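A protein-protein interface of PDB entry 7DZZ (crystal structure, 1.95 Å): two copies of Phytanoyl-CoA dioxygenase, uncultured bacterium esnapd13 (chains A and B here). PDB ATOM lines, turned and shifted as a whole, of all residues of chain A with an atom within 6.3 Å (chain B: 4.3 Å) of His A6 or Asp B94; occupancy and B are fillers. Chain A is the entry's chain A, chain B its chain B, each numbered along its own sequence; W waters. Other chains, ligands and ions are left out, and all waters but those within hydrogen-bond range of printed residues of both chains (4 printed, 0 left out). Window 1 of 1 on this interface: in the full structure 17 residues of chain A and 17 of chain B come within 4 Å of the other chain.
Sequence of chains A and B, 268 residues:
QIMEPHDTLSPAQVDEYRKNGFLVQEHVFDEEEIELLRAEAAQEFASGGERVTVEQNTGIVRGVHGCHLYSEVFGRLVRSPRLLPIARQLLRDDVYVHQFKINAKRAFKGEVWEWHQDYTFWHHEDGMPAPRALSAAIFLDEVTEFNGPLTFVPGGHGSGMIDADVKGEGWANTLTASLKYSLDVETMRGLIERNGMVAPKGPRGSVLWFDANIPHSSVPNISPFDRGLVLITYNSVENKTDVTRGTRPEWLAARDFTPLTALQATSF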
ATOM      1  N   MET A   3      20.235 -27.953  -7.643  1.00  0.00           N
ATOM      2  CA  MET A   3      19.882 -27.335  -6.380  1.00  0.00           C
ATOM      3  C   MET A   3      18.586 -27.971  -5.919  1.00  0.00           C
ATOM      4  O   MET A   3      17.654 -28.168  -6.690  1.00  0.00           O
ATOM      5  CB  MET A   3      19.657 -25.816  -6.498  1.00  0.00           C
ATOM      6  CG  MET A   3      20.889 -24.958  -6.568  1.00  0.00           C
ATOM      7  SD  MET A   3      21.913 -24.951  -5.086  1.00  0.00           S
ATOM      8  CE  MET A   3      23.084 -23.711  -5.605  1.00  0.00           C
ATOM      9  N   GLU A   4      18.469 -28.224  -4.638  1.00  0.00           N
ATOM     10  CA  GLU A   4      17.190 -28.692  -4.117  1.00  0.00           C
ATOM     11  C   GLU A   4      16.083 -27.713  -4.431  1.00  0.00           C
ATOM     12  O   GLU A   4      16.286 -26.495  -4.290  1.00  0.00           O
ATOM     13  CB  GLU A   4      17.233 -28.870  -2.576  1.00  0.00           C
ATOM     14  CG  GLU A   4      18.052 -30.084  -2.071  1.00  0.00           C
ATOM     15  CD  GLU A   4      18.509 -29.845  -0.637  1.00  0.00           C
ATOM     16  OE1 GLU A   4      19.723 -29.880  -0.382  1.00  0.00           O
ATOM     17  OE2 GLU A   4      17.663 -29.489   0.233  1.00  0.00           O
ATOM     18  N   PRO A   5      14.902 -28.216  -4.783  1.00  0.00           N
ATOM     19  CA  PRO A   5      13.783 -27.304  -5.098  1.00  0.00           C
ATOM     20  C   PRO A   5      13.481 -26.356  -3.933  1.00  0.00           C
ATOM     21  O   PRO A   5      13.649 -26.711  -2.775  1.00  0.00           O
ATOM     22  CB  PRO A   5      12.623 -28.248  -5.357  1.00  0.00           C
ATOM     23  CG  PRO A   5      13.252 -29.563  -5.768  1.00  0.00           C
ATOM     24  CD  PRO A   5      14.607 -29.637  -5.124  1.00  0.00           C
ATOM     25  N   HIS A   6      13.114 -25.122  -4.243  1.00  0.00           N
ATOM     26  CA  HIS A   6      12.985 -24.089  -3.237  1.00  0.00           C
ATOM     27  C   HIS A   6      11.970 -24.519  -2.184  1.00  0.00           C
ATOM     28  O   HIS A   6      10.919 -25.077  -2.538  1.00  0.00           O
ATOM     29  CB  HIS A   6      12.513 -22.764  -3.833  1.00  0.00           C
ATOM     30  CG  HIS A   6      13.510 -22.092  -4.733  1.00  0.00           C
ATOM     31  ND1 HIS A   6      13.178 -21.017  -5.521  1.00  0.00           N
ATOM     32  CD2 HIS A   6      14.789 -22.381  -5.020  1.00  0.00           C
ATOM     33  CE1 HIS A   6      14.218 -20.669  -6.251  1.00  0.00           C
ATOM     34  NE2 HIS A   6      15.207 -21.479  -5.959  1.00  0.00           N
ATOM     35  N   ASP A   7      12.316 -24.327  -0.918  1.00  0.00           N
ATOM     36  CA  ASP A   7      11.449 -24.695   0.223  1.00  0.00           C
ATOM     37  C   ASP A   7      10.952 -23.400   0.742  1.00  0.00           C
ATOM     38  O   ASP A   7      11.717 -22.434   0.820  1.00  0.00           O
ATOM     39  CB  ASP A   7      12.220 -25.317   1.396  1.00  0.00           C
ATOM     40  CG  ASP A   7      12.569 -26.740   1.196  1.00  0.00           C
ATOM     41  OD1 ASP A   7      11.848 -27.448   0.447  1.00  0.00           O
ATOM     42  OD2 ASP A   7      13.598 -27.157   1.809  1.00  0.00           O
ATOM     43  N   THR A   8       9.661 -23.289   0.953  1.00  0.00           N
ATOM     44  CA  THR A   8       9.105 -22.105   1.609  1.00  0.00           C
ATOM     45  C   THR A   8       8.548 -22.463   2.975  1.00  0.00           C
ATOM     46  O   THR A   8       8.446 -23.649   3.271  1.00  0.00           O
ATOM     47  CB  THR A   8       7.985 -21.551   0.740  1.00  0.00           C
ATOM     48  OG1 THR A   8       7.326 -22.643   0.128  1.00  0.00           O
ATOM     49  CG2 THR A   8       8.601 -20.682  -0.346  1.00  0.00           C
ATOM     50  N   PRO A  81      19.233 -20.382  -2.213  1.00  0.00           N
ATOM     51  CA  PRO A  81      17.902 -20.945  -2.281  1.00  0.00           C
ATOM     52  C   PRO A  81      17.377 -21.345  -0.925  1.00  0.00           C
ATOM     53  O   PRO A  81      16.213 -21.635  -0.818  1.00  0.00           O
ATOM     54  CB  PRO A  81      18.058 -22.133  -3.260  1.00  0.00           C
ATOM     55  CG  PRO A  81      19.478 -22.471  -3.163  1.00  0.00           C
ATOM     56  CD  PRO A  81      20.187 -21.169  -2.988  1.00  0.00           C
ATOM     57  N   ARG A  82      18.194 -21.316   0.109  1.00  0.00           N
ATOM     58  CA  ARG A  82      17.667 -21.520   1.450  1.00  0.00           C
ATOM     59  C   ARG A  82      17.069 -20.270   2.009  1.00  0.00           C
ATOM     60  O   ARG A  82      16.450 -20.320   3.052  1.00  0.00           O
ATOM     61  CB  ARG A  82      18.836 -21.861   2.380  1.00  0.00           C
ATOM     62  CG  ARG A  82      19.671 -23.078   1.959  1.00  0.00           C
ATOM     63  CD  ARG A  82      18.940 -24.343   2.124  1.00  0.00           C
ATOM     64  NE  ARG A  82      19.892 -25.462   2.064  1.00  0.00           N
ATOM     65  CZ  ARG A  82      19.607 -26.679   1.582  1.00  0.00           C
ATOM     66  NH1 ARG A  82      18.398 -26.940   1.102  1.00  0.00           N
ATOM     67  NH2 ARG A  82      20.535 -27.649   1.578  1.00  0.00           N
ATOM     68  N   LEU A  84      16.452 -16.847  -0.135  1.00  0.00           N
ATOM     69  CA  LEU A  84      15.760 -15.932  -0.998  1.00  0.00           C
ATOM     70  C   LEU A  84      14.288 -16.301  -1.182  1.00  0.00           C
ATOM     71  O   LEU A  84      13.466 -15.418  -1.183  1.00  0.00           O
ATOM     72  CB  LEU A  84      16.468 -15.838  -2.367  1.00  0.00           C
ATOM     73  CG  LEU A  84      15.835 -14.900  -3.379  1.00  0.00           C
ATOM     74  CD1 LEU A  84      15.881 -13.483  -2.860  1.00  0.00           C
ATOM     75  CD2 LEU A  84      16.666 -14.998  -4.659  1.00  0.00           C
ATOM     76  N   PRO A  85      13.957 -17.567  -1.361  1.00  0.00           N
ATOM     77  CA  PRO A  85      12.526 -17.858  -1.454  1.00  0.00           C
ATOM     78  C   PRO A  85      11.605 -17.506  -0.264  1.00  0.00           C
ATOM     79  O   PRO A  85      10.458 -17.124  -0.460  1.00  0.00           O
ATOM     80  CB  PRO A  85      12.497 -19.365  -1.762  1.00  0.00           C
ATOM     81  CG  PRO A  85      13.868 -19.673  -2.265  1.00  0.00           C
ATOM     82  CD  PRO A  85      14.745 -18.786  -1.473  1.00  0.00           C
ATOM     83  N   ARG A  88      11.202 -13.607  -0.260  1.00  0.00           N
ATOM     84  CA  ARG A  88      10.114 -13.354  -1.206  1.00  0.00           C
ATOM     85  C   ARG A  88       8.686 -13.680  -0.726  1.00  0.00           C
ATOM     86  O   ARG A  88       7.738 -12.889  -0.903  1.00  0.00           O
ATOM     87  CB  ARG A  88      10.372 -14.178  -2.459  1.00  0.00           C
ATOM     88  CG  ARG A  88      11.509 -13.642  -3.320  1.00  0.00           C
ATOM     89  CD  ARG A  88      11.764 -14.607  -4.432  1.00  0.00           C
ATOM     90  NE  ARG A  88      12.739 -14.136  -5.445  1.00  0.00           N
ATOM     91  CZ  ARG A  88      13.076 -14.837  -6.503  1.00  0.00           C
ATOM     92  NH1 ARG A  88      12.508 -15.985  -6.719  1.00  0.00           N
ATOM     93  NH2 ARG A  88      13.947 -14.352  -7.407  1.00  0.00           N
ATOM     94  N   ASP A  94       9.351  -9.389  -4.959  1.00  0.00           N
ATOM     95  CA  ASP A  94      10.768  -9.500  -5.149  1.00  0.00           C
ATOM     96  C   ASP A  94      11.451  -8.675  -4.027  1.00  0.00           C
ATOM     97  O   ASP A  94      10.843  -7.714  -3.474  1.00  0.00           O
ATOM     98  CB  ASP A  94      11.210  -8.986  -6.489  1.00  0.00           C
ATOM     99  CG  ASP A  94      11.086 -10.021  -7.617  1.00  0.00           C
ATOM    100  OD1 ASP A  94      11.382 -11.241  -7.416  1.00  0.00           O
ATOM    101  OD2 ASP A  94      10.743  -9.568  -8.771  1.00  0.00           O
ATOM    102  N   LEU A 260      16.703  -9.563  -6.541  1.00  0.00           N
ATOM    103  CA  LEU A 260      17.583 -10.664  -6.498  1.00  0.00           C
ATOM    104  C   LEU A 260      16.986 -11.905  -7.185  1.00  0.00           C
ATOM    105  O   LEU A 260      15.802 -12.127  -7.080  1.00  0.00           O
ATOM    106  CB  LEU A 260      17.843 -11.083  -5.036  1.00  0.00           C
ATOM    107  CG  LEU A 260      18.695 -10.005  -4.313  1.00  0.00           C
ATOM    108  CD1 LEU A 260      18.585 -10.232  -2.804  1.00  0.00           C
ATOM    109  CD2 LEU A 260      20.133 -10.051  -4.740  1.00  0.00           C
ATOM    110  N   THR A 261      17.873 -12.710  -7.738  1.00  0.00           N
ATOM    111  CA  THR A 261      17.595 -14.006  -8.310  1.00  0.00           C
ATOM    112  C   THR A 261      18.327 -15.084  -7.553  1.00  0.00           C
ATOM    113  O   THR A 261      19.381 -14.868  -6.984  1.00  0.00           O
ATOM    114  CB  THR A 261      18.080 -14.074  -9.837  1.00  0.00           C
ATOM    115  OG1 THR A 261      19.485 -14.019  -9.869  1.00  0.00           O
ATOM    116  CG2 THR A 261      17.642 -13.012 -10.608  1.00  0.00           C
ATOM    117  N   ALA A 262      17.788 -16.280  -7.543  1.00  0.00           N
ATOM    118  CA  ALA A 262      18.398 -17.378  -6.804  1.00  0.00           C
ATOM    119  C   ALA A 262      19.625 -17.943  -7.498  1.00  0.00           C
ATOM    120  O   ALA A 262      19.749 -17.928  -8.726  1.00  0.00           O
ATOM    121  CB  ALA A 262      17.422 -18.489  -6.621  1.00  0.00           C
ATOM    122  N   LEU A 263      20.515 -18.437  -6.676  1.00  0.00           N
ATOM    123  CA  LEU A 263      21.706 -19.116  -7.159  1.00  0.00           C
ATOM    124  C   LEU A 263      21.292 -20.456  -7.757  1.00  0.00           C
ATOM    125  O   LEU A 263      20.502 -21.195  -7.171  1.00  0.00           O
ATOM    126  CB  LEU A 263      22.530 -19.442  -5.965  1.00  0.00           C
ATOM    127  CG  LEU A 263      23.927 -19.074  -5.849  1.00  0.00           C
ATOM    128  CD1 LEU A 263      24.009 -17.572  -5.827  1.00  0.00           C
ATOM    129  CD2 LEU A 263      24.391 -19.686  -4.512  1.00  0.00           C
ATOM    130  N   GLN A 264      21.812 -20.748  -8.940  1.00  0.00           N
ATOM    131  CA  GLN A 264      21.661 -22.029  -9.592  1.00  0.00           C
ATOM    132  C   GLN A 264      22.971 -22.861  -9.462  1.00  0.00           C
ATOM    133  O   GLN A 264      24.024 -22.321  -9.166  1.00  0.00           O
ATOM    134  CB  GLN A 264      21.393 -21.782 -11.071  1.00  0.00           C
ATOM    135  CG  GLN A 264      20.054 -21.148 -11.353  1.00  0.00           C
ATOM    136  CD  GLN A 264      18.825 -21.938 -10.932  1.00  0.00           C
ATOM    137  OE1 GLN A 264      18.828 -23.158 -10.766  1.00  0.00           O
ATOM    138  NE2 GLN A 264      17.740 -21.175 -10.658  1.00  0.00           N
ATOM    139  N   ARG B  88       6.655 -19.492  -9.984  1.00  0.00           N
ATOM    140  CA  ARG B  88       7.837 -19.735  -9.129  1.00  0.00           C
ATOM    141  C   ARG B  88       7.495 -20.716  -8.000  1.00  0.00           C
ATOM    142  O   ARG B  88       8.269 -21.625  -7.689  1.00  0.00           O
ATOM    143  CB  ARG B  88       8.320 -18.420  -8.495  1.00  0.00           C
ATOM    144  CG  ARG B  88       9.007 -17.457  -9.410  1.00  0.00           C
ATOM    145  CD  ARG B  88       9.229 -16.088  -8.697  1.00  0.00           C
ATOM    146  NE  ARG B  88      10.123 -15.137  -9.389  1.00  0.00           N
ATOM    147  CZ  ARG B  88      10.426 -13.979  -8.845  1.00  0.00           C
ATOM    148  NH1 ARG B  88       9.902 -13.625  -7.672  1.00  0.00           N
ATOM    149  NH2 ARG B  88      11.207 -13.152  -9.448  1.00  0.00           N
ATOM    150  N   ARG B  92       8.970 -24.312  -7.967  1.00  0.00           N
ATOM    151  CA  ARG B  92       9.925 -24.238  -6.873  1.00  0.00           C
ATOM    152  C   ARG B  92      11.288 -23.791  -7.361  1.00  0.00           C
ATOM    153  O   ARG B  92      12.329 -24.383  -6.988  1.00  0.00           O
ATOM    154  CB  ARG B  92       9.973 -25.592  -6.102  1.00  0.00           C
ATOM    155  CG  ARG B  92       8.582 -26.045  -5.631  1.00  0.00           C
ATOM    156  CD  ARG B  92       8.581 -27.388  -4.929  1.00  0.00           C
ATOM    157  NE  ARG B  92       9.399 -27.324  -3.710  1.00  0.00           N
ATOM    158  CZ  ARG B  92       9.685 -28.367  -2.920  1.00  0.00           C
ATOM    159  NH1 ARG B  92       9.285 -29.597  -3.239  1.00  0.00           N
ATOM    160  NH2 ARG B  92      10.440 -28.187  -1.847  1.00  0.00           N
ATOM    161  N   ASP B  93      11.297 -22.732  -8.189  1.00  0.00           N
ATOM    162  CA  ASP B  93      12.517 -22.179  -8.778  1.00  0.00           C
ATOM    163  C   ASP B  93      12.232 -20.817  -9.257  1.00  0.00           C
ATOM    164  O   ASP B  93      11.078 -20.353  -9.246  1.00  0.00           O
ATOM    165  CB  ASP B  93      12.896 -23.024 -10.018  1.00  0.00           C
ATOM    166  CG  ASP B  93      14.334 -22.919 -10.417  1.00  0.00           C
ATOM    167  OD1 ASP B  93      15.157 -22.164  -9.814  1.00  0.00           O
ATOM    168  OD2 ASP B  93      14.662 -23.689 -11.349  1.00  0.00           O
ATOM    169  N   ASP B  94      13.277 -20.140  -9.687  1.00  0.00           N
ATOM    170  CA  ASP B  94      13.116 -19.043 -10.606  1.00  0.00           C
ATOM    171  C   ASP B  94      12.655 -19.647 -11.919  1.00  0.00           C
ATOM    172  O   ASP B  94      12.873 -20.844 -12.180  1.00  0.00           O
ATOM    173  CB  ASP B  94      14.406 -18.269 -10.868  1.00  0.00           C
ATOM    174  CG  ASP B  94      14.649 -17.153  -9.860  1.00  0.00           C
ATOM    175  OD1 ASP B  94      13.670 -16.405  -9.489  1.00  0.00           O
ATOM    176  OD2 ASP B  94      15.856 -17.001  -9.496  1.00  0.00           O
ATOM    177  N   VAL B  95      12.014 -18.833 -12.714  1.00  0.00           N
ATOM    178  CA  VAL B  95      11.475 -19.255 -13.980  1.00  0.00           C
ATOM    179  C   VAL B  95      11.749 -18.330 -15.114  1.00  0.00           C
ATOM    180  O   VAL B  95      12.093 -17.159 -14.943  1.00  0.00           O
ATOM    181  CB  VAL B  95       9.928 -19.429 -13.907  1.00  0.00           C
ATOM    182  CG1 VAL B  95       9.528 -20.514 -12.875  1.00  0.00           C
ATOM    183  CG2 VAL B  95       9.266 -18.132 -13.560  1.00  0.00           C
ATOM    184  N   ASN B 235       9.024 -22.411 -17.540  1.00  0.00           N
ATOM    185  CA  ASN B 235       9.923 -23.474 -17.187  1.00  0.00           C
ATOM    186  C   ASN B 235      10.868 -22.993 -16.041  1.00  0.00           C
ATOM    187  O   ASN B 235      11.313 -21.831 -15.980  1.00  0.00           O
ATOM    188  CB  ASN B 235      10.771 -23.819 -18.428  1.00  0.00           C
ATOM    189  CG  ASN B 235      11.545 -25.094 -18.248  1.00  0.00           C
ATOM    190  OD1 ASN B 235      11.226 -25.913 -17.421  1.00  0.00           O
ATOM    191  ND2 ASN B 235      12.593 -25.226 -18.991  1.00  0.00           N
ATOM    192  N   SER B 236      11.183 -23.911 -15.167  1.00  0.00           N
ATOM    193  CA  SER B 236      12.201 -23.741 -14.148  1.00  0.00           C
ATOM    194  C   SER B 236      13.544 -23.428 -14.841  1.00  0.00           C
ATOM    195  O   SER B 236      13.881 -24.020 -15.841  1.00  0.00           O
ATOM    196  CB  SER B 236      12.328 -25.073 -13.391  1.00  0.00           C
ATOM    197  OG  SER B 236      13.682 -25.329 -13.003  1.00  0.00           O
ATOM    198  N   VAL B 237      14.296 -22.496 -14.280  1.00  0.00           N
ATOM    199  CA  VAL B 237      15.596 -22.111 -14.747  1.00  0.00           C
ATOM    200  C   VAL B 237      16.576 -23.255 -14.597  1.00  0.00           C
ATOM    201  O   VAL B 237      17.407 -23.429 -15.494  1.00  0.00           O
ATOM    202  CB  VAL B 237      16.081 -20.794 -14.055  1.00  0.00           C
ATOM    203  CG1 VAL B 237      17.553 -20.450 -14.303  1.00  0.00           C
ATOM    204  CG2 VAL B 237      15.283 -19.631 -14.641  1.00  0.00           C
ATOM    205  N   PRO B 259      16.388 -15.329 -15.334  1.00  0.00           N
ATOM    206  CA  PRO B 259      15.256 -15.392 -14.482  1.00  0.00           C
ATOM    207  C   PRO B 259      14.384 -14.194 -14.578  1.00  0.00           C
ATOM    208  O   PRO B 259      14.879 -13.023 -14.572  1.00  0.00           O
ATOM    209  CB  PRO B 259      15.866 -15.570 -13.057  1.00  0.00           C
ATOM    210  CG  PRO B 259      17.275 -15.689 -13.246  1.00  0.00           C
ATOM    211  CD  PRO B 259      17.672 -15.363 -14.596  1.00  0.00           C
HETATM  212  O   HOH W   1      10.597 -20.332  -5.991  1.00  0.00           O
HETATM  213  O   HOH W   2      17.971 -18.158 -10.649  1.00  0.00           O
HETATM  214  O   HOH W   3      13.532 -29.217  -1.388  1.00  0.00           O
HETATM  215  O   HOH W   4      16.982 -24.151  -8.658  1.00  0.00           O
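N of His A6 sits at hydrogen-bond distance from O of Arg B92 (2.9 Å).
The side-chain carboxylate (OD1) of Asp A7 is in salt-bridge range of the guanidinium group (NH2) of Arg B92, 2.8 Å away.
NH2 of Arg A88 lies within salt-bridge range of OD1 of Asp B94.
The guanidinium group (NH2) of Arg B88 is in salt-bridge range of the side-chain carboxylate (OD1) of Asp A94.
N of Ala A262 lies within hydrogen-bond range of OD2 of Asp B94 (2.8 Å).
OD1 of Asp B93 is in hydrogen-bond range of NE2 of Gln A264 (2.9 Å).
The backbone carbonyl oxygen (O) of Leu A260 sits at hydrogen-bond distance from the guanidinium group (NH2) of Arg A88, 2.9 Å away.
The backbone carbonyl oxygen of Arg B88 lies within hydrogen-bond range of the backbone NH of Asp B93.
OD1 of Asp B94 lies within salt-bridge range of NE of Arg B88, at 3.8 Å.
The side-chain hydroxyl (OG) of Ser B236 sits at hydrogen-bond distance from the side-chain carboxylate (OD2) of Asp B93, at 2.5 Å.
The backbone NH (N) of Val B237 sits at hydrogen-bond distance from the side-chain carboxylate (OD2) of Asp B93.
O of Asp B94 lies within hydrogen-bond range of N of Val B237 (3.0 Å).
Among the printed residues, pairs that only touch across the chains: His A6 with Asp B93 (3.4 Å), Arg A88 with Arg B88 (3.6 Å), His A6 with Asp B94 (3.6 Å), Pro A5 with Arg B92 (3.7 Å), Thr A261 with Asp B94 (3.7 Å), Gln A264 with Val B237 (3.7 Å) and Thr A261 with Pro B259 (3.8 Å).
His A6 touches just these residues of chain B: Arg B92 (2.9 Å), Asp B93 (3.4 Å) and Asp B94 (3.6 Å).
Asp B94 touches just these residues of chain A: His A6, Arg A88, Thr A261 and Ala A262.
Printed residues of chain A within 4 Å of Asp B93: His A6 and Gln A264.
Of the printed residues of chain B, Pro A5 touches Arg B92.
Of the printed residues of chain B, Arg A88 touches Arg B88 and Asp B94.
Of the printed residues of chain A, Val B237 touches Gln A264.
Arg A82 touches none of the printed residues of chain B.
Glu A4 touches none of the printed residues of chain B.
The nearest printed residue of chain B that does not touch His A6 is Arg B88 (5.4 Å).
Of the 17 printed residues of chain A, 8 touch a printed residue of chain B.
Hydrophobic or aromatic side chains of chain A that line the printed part of chain B: Pro A5, His A6 and Ala A262.
Arg A88 touches its own counterpart, Arg B88.
Arg A88 touches Asp B94, and with the chains exchanged Asp A94 touches Arg B88.
Water W2 lies within hydrogen-bond range of the backbone carbonyl oxygen (O) of Ala A262, the side-chain carboxylate (OD2) of Asp B94 and the side-chain amide nitrogen (NE2) of Gln A264.
Water W1 lies within hydrogen-bond range of a ring nitrogen (ND1) of His A6 (2.7 Å), the backbone carbonyl oxygen (O) of Arg B88 (3.2 Å) and the backbone carbonyl oxygen (O) of Asp B93 (3.3 Å).
Water W3 lies within hydrogen-bond range of the backbone carbonyl oxygen of Pro A5 (2.9 Å), the side-chain carboxylate of Asp A7 (3.1 Å) and the guanidinium group of Arg B92 (3.3 Å).
Water W4 lies within hydrogen-bond range of OD1 of Asp B93 (2.9 Å) and OE1 of Gln A264 (3.0 Å).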
